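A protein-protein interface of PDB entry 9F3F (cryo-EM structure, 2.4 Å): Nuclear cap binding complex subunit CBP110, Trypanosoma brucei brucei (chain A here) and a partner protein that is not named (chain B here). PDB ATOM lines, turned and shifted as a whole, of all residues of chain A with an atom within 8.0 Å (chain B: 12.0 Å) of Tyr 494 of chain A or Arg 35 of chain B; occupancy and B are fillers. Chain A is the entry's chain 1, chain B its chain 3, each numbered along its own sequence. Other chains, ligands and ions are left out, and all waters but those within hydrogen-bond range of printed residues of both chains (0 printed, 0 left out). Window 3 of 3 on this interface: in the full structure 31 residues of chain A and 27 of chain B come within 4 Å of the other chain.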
ATOM      1  N   PHE A 446      19.845  18.388  -3.541  1.00  0.00           N
ATOM      2  CA  PHE A 446      19.718  19.841  -3.847  1.00  0.00           C
ATOM      3  C   PHE A 446      18.712  20.059  -4.974  1.00  0.00           C
ATOM      4  O   PHE A 446      18.844  21.050  -5.705  1.00  0.00           O
ATOM      5  CB  PHE A 446      21.102  20.439  -4.102  1.00  0.00           C
ATOM      6  CG  PHE A 446      22.053  20.394  -2.936  1.00  0.00           C
ATOM      7  CD1 PHE A 446      21.762  21.052  -1.756  1.00  0.00           C
ATOM      8  CD2 PHE A 446      23.228  19.666  -3.012  1.00  0.00           C
ATOM      9  CE1 PHE A 446      22.641  21.011  -0.687  1.00  0.00           C
ATOM     10  CE2 PHE A 446      24.099  19.615  -1.938  1.00  0.00           C
ATOM     11  CZ  PHE A 446      23.807  20.291  -0.780  1.00  0.00           C
ATOM     12  N   VAL A 489      23.066  26.631   1.475  1.00  0.00           N
ATOM     13  CA  VAL A 489      23.179  25.392   0.716  1.00  0.00           C
ATOM     14  C   VAL A 489      24.569  25.252   0.109  1.00  0.00           C
ATOM     15  O   VAL A 489      25.145  24.160   0.095  1.00  0.00           O
ATOM     16  CB  VAL A 489      22.075  25.343  -0.357  1.00  0.00           C
ATOM     17  CG1 VAL A 489      22.503  24.503  -1.542  1.00  0.00           C
ATOM     18  CG2 VAL A 489      20.785  24.821   0.239  1.00  0.00           C
ATOM     19  N   ALA A 490      25.136  26.355  -0.385  1.00  0.00           N
ATOM     20  CA  ALA A 490      26.425  26.299  -1.066  1.00  0.00           C
ATOM     21  C   ALA A 490      27.556  25.846  -0.153  1.00  0.00           C
ATOM     22  O   ALA A 490      28.593  25.402  -0.653  1.00  0.00           O
ATOM     23  CB  ALA A 490      26.767  27.662  -1.664  1.00  0.00           C
ATOM     24  N   ARG A 491      27.379  25.927   1.165  1.00  0.00           N
ATOM     25  CA  ARG A 491      28.424  25.476   2.123  1.00  0.00           C
ATOM     26  C   ARG A 491      28.493  23.942   2.141  1.00  0.00           C
ATOM     27  O   ARG A 491      29.579  23.406   2.414  1.00  0.00           O
ATOM     28  CB  ARG A 491      28.173  26.066   3.512  1.00  0.00           C
ATOM     29  CG  ARG A 491      28.042  27.577   3.593  1.00  0.00           C
ATOM     30  CD  ARG A 491      27.831  27.968   5.036  1.00  0.00           C
ATOM     31  NE  ARG A 491      27.305  29.331   5.152  1.00  0.00           N
ATOM     32  CZ  ARG A 491      26.163  29.621   5.752  1.00  0.00           C
ATOM     33  NH1 ARG A 491      25.518  28.685   6.422  1.00  0.00           N
ATOM     34  NH2 ARG A 491      25.675  30.847   5.689  1.00  0.00           N
ATOM     35  N   ARG A 492      27.389  23.268   1.834  1.00  0.00           N
ATOM     36  CA  ARG A 492      27.348  21.814   1.819  1.00  0.00           C
ATOM     37  C   ARG A 492      27.708  21.223   0.466  1.00  0.00           C
ATOM     38  O   ARG A 492      27.741  19.995   0.334  1.00  0.00           O
ATOM     39  CB  ARG A 492      25.959  21.324   2.232  1.00  0.00           C
ATOM     40  CG  ARG A 492      25.238  22.233   3.199  1.00  0.00           C
ATOM     41  CD  ARG A 492      23.995  21.560   3.729  1.00  0.00           C
ATOM     42  NE  ARG A 492      23.688  21.961   5.093  1.00  0.00           N
ATOM     43  CZ  ARG A 492      23.421  21.114   6.076  1.00  0.00           C
ATOM     44  NH1 ARG A 492      23.423  19.806   5.880  1.00  0.00           N
ATOM     45  NH2 ARG A 492      23.146  21.591   7.287  1.00  0.00           N
ATOM     46  N   THR A 493      27.978  22.050  -0.533  1.00  0.00           N
ATOM     47  CA  THR A 493      28.292  21.562  -1.869  1.00  0.00           C
ATOM     48  C   THR A 493      29.291  22.524  -2.494  1.00  0.00           C
ATOM     49  O   THR A 493      29.944  23.304  -1.794  1.00  0.00           O
ATOM     50  CB  THR A 493      27.013  21.408  -2.710  1.00  0.00           C
ATOM     51  OG1 THR A 493      27.364  21.258  -4.091  1.00  0.00           O
ATOM     52  CG2 THR A 493      26.124  22.626  -2.560  1.00  0.00           C
ATOM     53  N   TYR A 494      29.432  22.455  -3.809  1.00  0.00           N
ATOM     54  CA  TYR A 494      30.295  23.354  -4.554  1.00  0.00           C
ATOM     55  C   TYR A 494      29.473  24.121  -5.580  1.00  0.00           C
ATOM     56  O   TYR A 494      28.297  23.832  -5.815  1.00  0.00           O
ATOM     57  CB  TYR A 494      31.445  22.597  -5.228  1.00  0.00           C
ATOM     58  CG  TYR A 494      31.075  21.291  -5.893  1.00  0.00           C
ATOM     59  CD1 TYR A 494      30.719  20.179  -5.148  1.00  0.00           C
ATOM     60  CD2 TYR A 494      31.123  21.162  -7.269  1.00  0.00           C
ATOM     61  CE1 TYR A 494      30.392  18.992  -5.753  1.00  0.00           C
ATOM     62  CE2 TYR A 494      30.807  19.974  -7.881  1.00  0.00           C
ATOM     63  CZ  TYR A 494      30.441  18.893  -7.119  1.00  0.00           C
ATOM     64  OH  TYR A 494      30.119  17.705  -7.728  1.00  0.00           O
ATOM     65  N   GLY A 495      30.110  25.123  -6.187  1.00  0.00           N
ATOM     66  CA  GLY A 495      29.399  26.006  -7.093  1.00  0.00           C
ATOM     67  C   GLY A 495      28.874  25.318  -8.334  1.00  0.00           C
ATOM     68  O   GLY A 495      27.813  25.684  -8.845  1.00  0.00           O
ATOM     69  N   LEU A 496      29.603  24.324  -8.839  1.00  0.00           N
ATOM     70  CA  LEU A 496      29.209  23.675 -10.084  1.00  0.00           C
ATOM     71  C   LEU A 496      27.899  22.910  -9.933  1.00  0.00           C
ATOM     72  O   LEU A 496      27.059  22.930 -10.840  1.00  0.00           O
ATOM     73  CB  LEU A 496      30.324  22.752 -10.564  1.00  0.00           C
ATOM     74  CG  LEU A 496      31.577  23.419 -11.130  1.00  0.00           C
ATOM     75  CD1 LEU A 496      32.229  22.522 -12.163  1.00  0.00           C
ATOM     76  CD2 LEU A 496      31.250  24.771 -11.734  1.00  0.00           C
ATOM     77  N   ARG A 497      27.708  22.221  -8.806  1.00  0.00           N
ATOM     78  CA  ARG A 497      26.471  21.472  -8.603  1.00  0.00           C
ATOM     79  C   ARG A 497      25.265  22.395  -8.557  1.00  0.00           C
ATOM     80  O   ARG A 497      24.236  22.119  -9.184  1.00  0.00           O
ATOM     81  CB  ARG A 497      26.553  20.647  -7.320  1.00  0.00           C
ATOM     82  CG  ARG A 497      27.159  19.272  -7.504  1.00  0.00           C
ATOM     83  CD  ARG A 497      26.115  18.224  -7.825  1.00  0.00           C
ATOM     84  NE  ARG A 497      24.920  18.368  -7.004  1.00  0.00           N
ATOM     85  CZ  ARG A 497      24.048  17.397  -6.781  1.00  0.00           C
ATOM     86  NH1 ARG A 497      24.227  16.184  -7.270  1.00  0.00           N
ATOM     87  NH2 ARG A 497      22.973  17.649  -6.041  1.00  0.00           N
ATOM     88  N   LEU A 498      25.370  23.497  -7.815  1.00  0.00           N
ATOM     89  CA  LEU A 498      24.266  24.443  -7.745  1.00  0.00           C
ATOM     90  C   LEU A 498      24.038  25.117  -9.091  1.00  0.00           C
ATOM     91  O   LEU A 498      22.893  25.398  -9.463  1.00  0.00           O
ATOM     92  CB  LEU A 498      24.534  25.479  -6.660  1.00  0.00           C
ATOM     93  CG  LEU A 498      24.022  25.136  -5.264  1.00  0.00           C
ATOM     94  CD1 LEU A 498      24.179  26.330  -4.343  1.00  0.00           C
ATOM     95  CD2 LEU A 498      22.576  24.692  -5.328  1.00  0.00           C
ATOM     96  N   ARG A 499      25.114  25.387  -9.831  1.00  0.00           N
ATOM     97  CA  ARG A 499      24.977  25.956 -11.166  1.00  0.00           C
ATOM     98  C   ARG A 499      24.202  25.016 -12.079  1.00  0.00           C
ATOM     99  O   ARG A 499      23.304  25.441 -12.813  1.00  0.00           O
ATOM    100  CB  ARG A 499      26.356  26.248 -11.754  1.00  0.00           C
ATOM    101  CG  ARG A 499      27.141  27.350 -11.057  1.00  0.00           C
ATOM    102  CD  ARG A 499      28.477  27.617 -11.725  1.00  0.00           C
ATOM    103  NE  ARG A 499      29.240  28.625 -11.001  1.00  0.00           N
ATOM    104  CZ  ARG A 499      30.486  28.974 -11.289  1.00  0.00           C
ATOM    105  NH1 ARG A 499      31.149  28.409 -12.286  1.00  0.00           N
ATOM    106  NH2 ARG A 499      31.082  29.912 -10.560  1.00  0.00           N
ATOM    107  N   ALA A 500      24.544  23.727 -12.046  1.00  0.00           N
ATOM    108  CA  ALA A 500      23.852  22.756 -12.884  1.00  0.00           C
ATOM    109  C   ALA A 500      22.396  22.595 -12.464  1.00  0.00           C
ATOM    110  O   ALA A 500      21.502  22.545 -13.315  1.00  0.00           O
ATOM    111  CB  ALA A 500      24.577  21.414 -12.838  1.00  0.00           C
ATOM    112  N   ILE A 513      25.699  35.039  -4.884  1.00  0.00           N
ATOM    113  CA  ILE A 513      26.222  34.103  -3.889  1.00  0.00           C
ATOM    114  C   ILE A 513      27.581  33.532  -4.269  1.00  0.00           C
ATOM    115  O   ILE A 513      28.189  32.824  -3.451  1.00  0.00           O
ATOM    116  CB  ILE A 513      25.242  32.941  -3.627  1.00  0.00           C
ATOM    117  CG1 ILE A 513      25.263  31.952  -4.792  1.00  0.00           C
ATOM    118  CG2 ILE A 513      23.836  33.468  -3.389  1.00  0.00           C
ATOM    119  CD1 ILE A 513      24.568  30.648  -4.495  1.00  0.00           C
ATOM    120  N   PHE A 514      28.075  33.809  -5.469  1.00  0.00           N
ATOM    121  CA  PHE A 514      29.394  33.339  -5.870  1.00  0.00           C
ATOM    122  C   PHE A 514      30.220  34.454  -6.502  1.00  0.00           C
ATOM    123  O   PHE A 514      29.893  35.634  -6.379  1.00  0.00           O
ATOM    124  CB  PHE A 514      29.274  32.164  -6.837  1.00  0.00           C
ATOM    125  CG  PHE A 514      28.842  30.888  -6.186  1.00  0.00           C
ATOM    126  CD1 PHE A 514      29.574  30.346  -5.144  1.00  0.00           C
ATOM    127  CD2 PHE A 514      27.711  30.221  -6.621  1.00  0.00           C
ATOM    128  CE1 PHE A 514      29.181  29.166  -4.543  1.00  0.00           C
ATOM    129  CE2 PHE A 514      27.313  29.042  -6.024  1.00  0.00           C
ATOM    130  CZ  PHE A 514      28.049  28.514  -4.984  1.00  0.00           C
ATOM    131  N   ARG B  33      35.501  14.053 -17.016  1.00  0.00           N
ATOM    132  CA  ARG B  33      35.844  13.625 -15.666  1.00  0.00           C
ATOM    133  C   ARG B  33      35.439  14.685 -14.649  1.00  0.00           C
ATOM    134  O   ARG B  33      35.990  14.754 -13.552  1.00  0.00           O
ATOM    135  CB  ARG B  33      37.341  13.333 -15.564  1.00  0.00           C
ATOM    136  CG  ARG B  33      37.796  12.148 -16.399  1.00  0.00           C
ATOM    137  CD  ARG B  33      38.875  11.347 -15.692  1.00  0.00           C
ATOM    138  NE  ARG B  33      38.399  10.780 -14.435  1.00  0.00           N
ATOM    139  CZ  ARG B  33      39.137  10.038 -13.620  1.00  0.00           C
ATOM    140  NH1 ARG B  33      40.397   9.750 -13.899  1.00  0.00           N
ATOM    141  NH2 ARG B  33      38.595   9.572 -12.499  1.00  0.00           N
ATOM    142  N   ARG B  34      34.467  15.508 -15.030  1.00  0.00           N
ATOM    143  CA  ARG B  34      33.983  16.578 -14.176  1.00  0.00           C
ATOM    144  C   ARG B  34      33.266  15.992 -12.959  1.00  0.00           C
ATOM    145  O   ARG B  34      32.725  14.884 -12.993  1.00  0.00           O
ATOM    146  CB  ARG B  34      33.072  17.508 -14.983  1.00  0.00           C
ATOM    147  CG  ARG B  34      32.242  18.496 -14.178  1.00  0.00           C
ATOM    148  CD  ARG B  34      30.886  18.720 -14.829  1.00  0.00           C
ATOM    149  NE  ARG B  34      30.258  17.464 -15.221  1.00  0.00           N
ATOM    150  CZ  ARG B  34      29.094  17.373 -15.851  1.00  0.00           C
ATOM    151  NH1 ARG B  34      28.398  18.450 -16.176  1.00  0.00           N
ATOM    152  NH2 ARG B  34      28.617  16.170 -16.161  1.00  0.00           N
ATOM    153  N   ARG B  35      33.280  16.754 -11.862  1.00  0.00           N
ATOM    154  CA  ARG B  35      32.748  16.263 -10.595  1.00  0.00           C
ATOM    155  C   ARG B  35      31.266  15.916 -10.684  1.00  0.00           C
ATOM    156  O   ARG B  35      30.788  15.066  -9.925  1.00  0.00           O
ATOM    157  CB  ARG B  35      32.988  17.298  -9.499  1.00  0.00           C
ATOM    158  CG  ARG B  35      33.303  16.711  -8.137  1.00  0.00           C
ATOM    159  CD  ARG B  35      33.675  17.804  -7.159  1.00  0.00           C
ATOM    160  NE  ARG B  35      33.394  17.433  -5.779  1.00  0.00           N
ATOM    161  CZ  ARG B  35      33.518  18.253  -4.746  1.00  0.00           C
ATOM    162  NH1 ARG B  35      33.917  19.503  -4.900  1.00  0.00           N
ATOM    163  NH2 ARG B  35      33.235  17.808  -3.527  1.00  0.00           N
ATOM    164  N   GLU B  36      30.520  16.559 -11.585  1.00  0.00           N
ATOM    165  CA  GLU B  36      29.113  16.206 -11.750  1.00  0.00           C
ATOM    166  C   GLU B  36      28.953  14.915 -12.538  1.00  0.00           C
ATOM    167  O   GLU B  36      27.994  14.165 -12.320  1.00  0.00           O
ATOM    168  CB  GLU B  36      28.358  17.339 -12.436  1.00  0.00           C
ATOM    169  CG  GLU B  36      27.895  18.414 -11.491  1.00  0.00           C
ATOM    170  CD  GLU B  36      29.026  19.303 -11.050  1.00  0.00           C
ATOM    171  OE1 GLU B  36      30.112  19.243 -11.665  1.00  0.00           O
ATOM    172  OE2 GLU B  36      28.831  20.062 -10.088  1.00  0.00           O
ATOM    173  N   GLU B  37      29.872  14.641 -13.464  1.00  0.00           N
ATOM    174  CA  GLU B  37      29.806  13.406 -14.233  1.00  0.00           C
ATOM    175  C   GLU B  37      29.941  12.174 -13.349  1.00  0.00           C
ATOM    176  O   GLU B  37      29.475  11.096 -13.732  1.00  0.00           O
ATOM    177  CB  GLU B  37      30.891  13.401 -15.312  1.00  0.00           C
ATOM    178  CG  GLU B  37      30.711  12.329 -16.380  1.00  0.00           C
ATOM    179  CD  GLU B  37      31.693  11.183 -16.228  1.00  0.00           C
ATOM    180  OE1 GLU B  37      32.864  11.442 -15.882  1.00  0.00           O
ATOM    181  OE2 GLU B  37      31.291  10.022 -16.450  1.00  0.00           O
ATOM    182  N   CYS B  38      30.557  12.309 -12.177  1.00  0.00           N
ATOM    183  CA  CYS B  38      30.743  11.197 -11.258  1.00  0.00           C
ATOM    184  C   CYS B  38      29.701  11.181 -10.146  1.00  0.00           C
ATOM    185  O   CYS B  38      29.923  10.559  -9.102  1.00  0.00           O
ATOM    186  CB  CYS B  38      32.156  11.231 -10.673  1.00  0.00           C
ATOM    187  SG  CYS B  38      32.428  12.451  -9.367  1.00  0.00           S
ATOM    188  N   VAL B  39      28.566  11.839 -10.354  1.00  0.00           N
ATOM    189  CA  VAL B  39      27.499  11.911  -9.364  1.00  0.00           C
ATOM    190  C   VAL B  39      26.365  10.999  -9.809  1.00  0.00           C
ATOM    191  O   VAL B  39      25.800  11.179 -10.893  1.00  0.00           O
ATOM    192  CB  VAL B  39      27.005  13.353  -9.177  1.00  0.00           C
ATOM    193  CG1 VAL B  39      25.676  13.365  -8.455  1.00  0.00           C
ATOM    194  CG2 VAL B  39      28.032  14.165  -8.413  1.00  0.00           C
ATOM    195  N   VAL B  40      26.040  10.015  -8.975  1.00  0.00           N
ATOM    196  CA  VAL B  40      24.924   9.101  -9.199  1.00  0.00           C
ATOM    197  C   VAL B  40      24.065   9.171  -7.945  1.00  0.00           C
ATOM    198  O   VAL B  40      24.533   8.873  -6.840  1.00  0.00           O
ATOM    199  CB  VAL B  40      25.388   7.670  -9.483  1.00  0.00           C
ATOM    200  CG1 VAL B  40      24.224   6.818  -9.932  1.00  0.00           C
ATOM    201  CG2 VAL B  40      26.494   7.665 -10.524  1.00  0.00           C
ATOM    202  N   LEU B  41      22.815   9.572  -8.106  1.00  0.00           N
ATOM    203  CA  LEU B  41      21.974   9.914  -6.977  1.00  0.00           C
ATOM    204  C   LEU B  41      21.280   8.643  -6.472  1.00  0.00           C
ATOM    205  O   LEU B  41      21.121   7.679  -7.223  1.00  0.00           O
ATOM    206  CB  LEU B  41      20.976  10.978  -7.423  1.00  0.00           C
ATOM    207  CG  LEU B  41      21.088  12.431  -6.923  1.00  0.00           C
ATOM    208  CD1 LEU B  41      19.769  13.179  -7.074  1.00  0.00           C
ATOM    209  CD2 LEU B  41      21.670  12.600  -5.529  1.00  0.00           C
ATOM    210  N   PRO B  77      20.568  20.458 -15.922  1.00  0.00           N
ATOM    211  CA  PRO B  77      20.870  19.025 -15.999  1.00  0.00           C
ATOM    212  C   PRO B  77      20.583  18.348 -14.670  1.00  0.00           C
ATOM    213  O   PRO B  77      20.804  18.916 -13.599  1.00  0.00           O
ATOM    214  CB  PRO B  77      22.362  18.986 -16.345  1.00  0.00           C
ATOM    215  CG  PRO B  77      22.683  20.347 -16.866  1.00  0.00           C
ATOM    216  CD  PRO B  77      21.763  21.285 -16.156  1.00  0.00           C
ATOM    217  N   ILE B  78      20.087  17.119 -14.748  1.00  0.00           N
ATOM    218  CA  ILE B  78      19.618  16.375 -13.589  1.00  0.00           C
ATOM    219  C   ILE B  78      20.458  15.113 -13.458  1.00  0.00           C
ATOM    220  O   ILE B  78      20.659  14.390 -14.441  1.00  0.00           O
ATOM    221  CB  ILE B  78      18.118  16.045 -13.711  1.00  0.00           C
ATOM    222  CG1 ILE B  78      17.276  17.202 -13.171  1.00  0.00           C
ATOM    223  CG2 ILE B  78      17.785  14.737 -13.031  1.00  0.00           C
ATOM    224  CD1 ILE B  78      17.770  17.761 -11.870  1.00  0.00           C
ATOM    225  N   LEU B  79      20.954  14.863 -12.253  1.00  0.00           N
ATOM    226  CA  LEU B  79      21.865  13.752 -12.039  1.00  0.00           C
ATOM    227  C   LEU B  79      21.121  12.426 -12.170  1.00  0.00           C
ATOM    228  O   LEU B  79      19.948  12.332 -11.800  1.00  0.00           O
ATOM    229  CB  LEU B  79      22.517  13.857 -10.664  1.00  0.00           C
ATOM    230  CG  LEU B  79      23.245  15.160 -10.318  1.00  0.00           C
ATOM    231  CD1 LEU B  79      24.108  15.642 -11.480  1.00  0.00           C
ATOM    232  CD2 LEU B  79      22.290  16.249  -9.840  1.00  0.00           C
ATOM    233  N   PRO B  80      21.771  11.390 -12.691  1.00  0.00           N
ATOM    234  CA  PRO B  80      21.092  10.110 -12.897  1.00  0.00           C
ATOM    235  C   PRO B  80      20.984   9.320 -11.607  1.00  0.00           C
ATOM    236  O   PRO B  80      21.993   9.076 -10.929  1.00  0.00           O
ATOM    237  CB  PRO B  80      21.996   9.398 -13.909  1.00  0.00           C
ATOM    238  CG  PRO B  80      23.337   9.958 -13.656  1.00  0.00           C
ATOM    239  CD  PRO B  80      23.132  11.387 -13.249  1.00  0.00           C
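Hydrophobic or aromatic side chains of chain A that line the printed part of chain B: Tyr 494 and Leu 496. Of the 13 printed residues of chain B, 5 touch a printed residue of chain A. Printed residues of chain B that touch a printed residue of chain A: Arg 35, Glu 36, Val 39, Pro 77 and Leu 79. Hydrophobic or aromatic side chains of chain B that line the printed part of chain A: Val 39, Pro 77 and Leu 79.
Among the printed residues, merely in contact across the chains: Tyr 494 of chain A with Glu 36 of chain B (3.0 Å), Arg 497 of chain A with Val 39 of chain B (3.4 Å) and Arg 497 of chain A with Leu 79 of chain B (3.2 Å).
N of Pro 77 of chain B lies close to O of Ala 500 of chain A (3.5 Å). The backbone carbonyl oxygen (O) of Leu 496 of chain A lies close to the side-chain carboxylate (OE2) of Glu 36 of chain B (3.5 Å). The side-chain carboxylate (OE2) of Glu 36 of chain B is in hydrogen-bond range of the backbone NH (N) of Arg 497 of chain A, at 2.8 Å. OH of Tyr 494 of chain A sits close to O of Arg 35 of chain B, at 3.5 Å.
No residue of chain B comes within 4 Å of Ala 490 of chain A. No residue of chain B comes within 4 Å of Thr 493 of chain A. Of chain B, only Arg 35 (3.3 Å) and Glu 36 (3.0 Å) come within 4 Å of Tyr 494 of chain A. No residue of chain B comes within 4 Å of Gly 495 of chain A. Arg 497 of chain A touches just these residues of chain B: Glu 36 (2.8 Å), Val 39 (3.4 Å) and Leu 79 (3.2 Å). No residue of chain B comes within 4 Å of Leu 498 of chain A. Arg 35 of chain B touches just one residue of chain A: Tyr 494 (3.3 Å). Of the printed residues of chain A, Glu 36 of chain B touches Tyr 494, Leu 496 and Arg 497. Cys 38 of chain B touches none of the printed residues of chain A. Of the printed residues of chain A, Pro 77 of chain B touches Ala 500 (3.1 Å). Of the printed residues of chain A, Leu 79 of chain B touches Arg 497 (3.2 Å). The nearest residue of chain B that does not touch Tyr 494 of chain A is Val 39 of chain B (4.2 Å). The nearest residue of chain A that does not touch Arg 35 of chain B is Leu 496 of chain A (5.9 Å). The nearest printed residue of chain A that does not touch Pro 77 of chain B is Arg 499 of chain A (5.6 Å).
The guanidinium group (NE) of Arg 34 of chain B lies within salt-bridge range of the side-chain carboxylate (OE1) of Glu 36 of chain B, 3.98 Å away. The backbone carbonyl oxygen (O) of Arg 35 of chain B sits at hydrogen-bond distance from the side-chain sulfur (SG) of Cys 38 of chain B.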
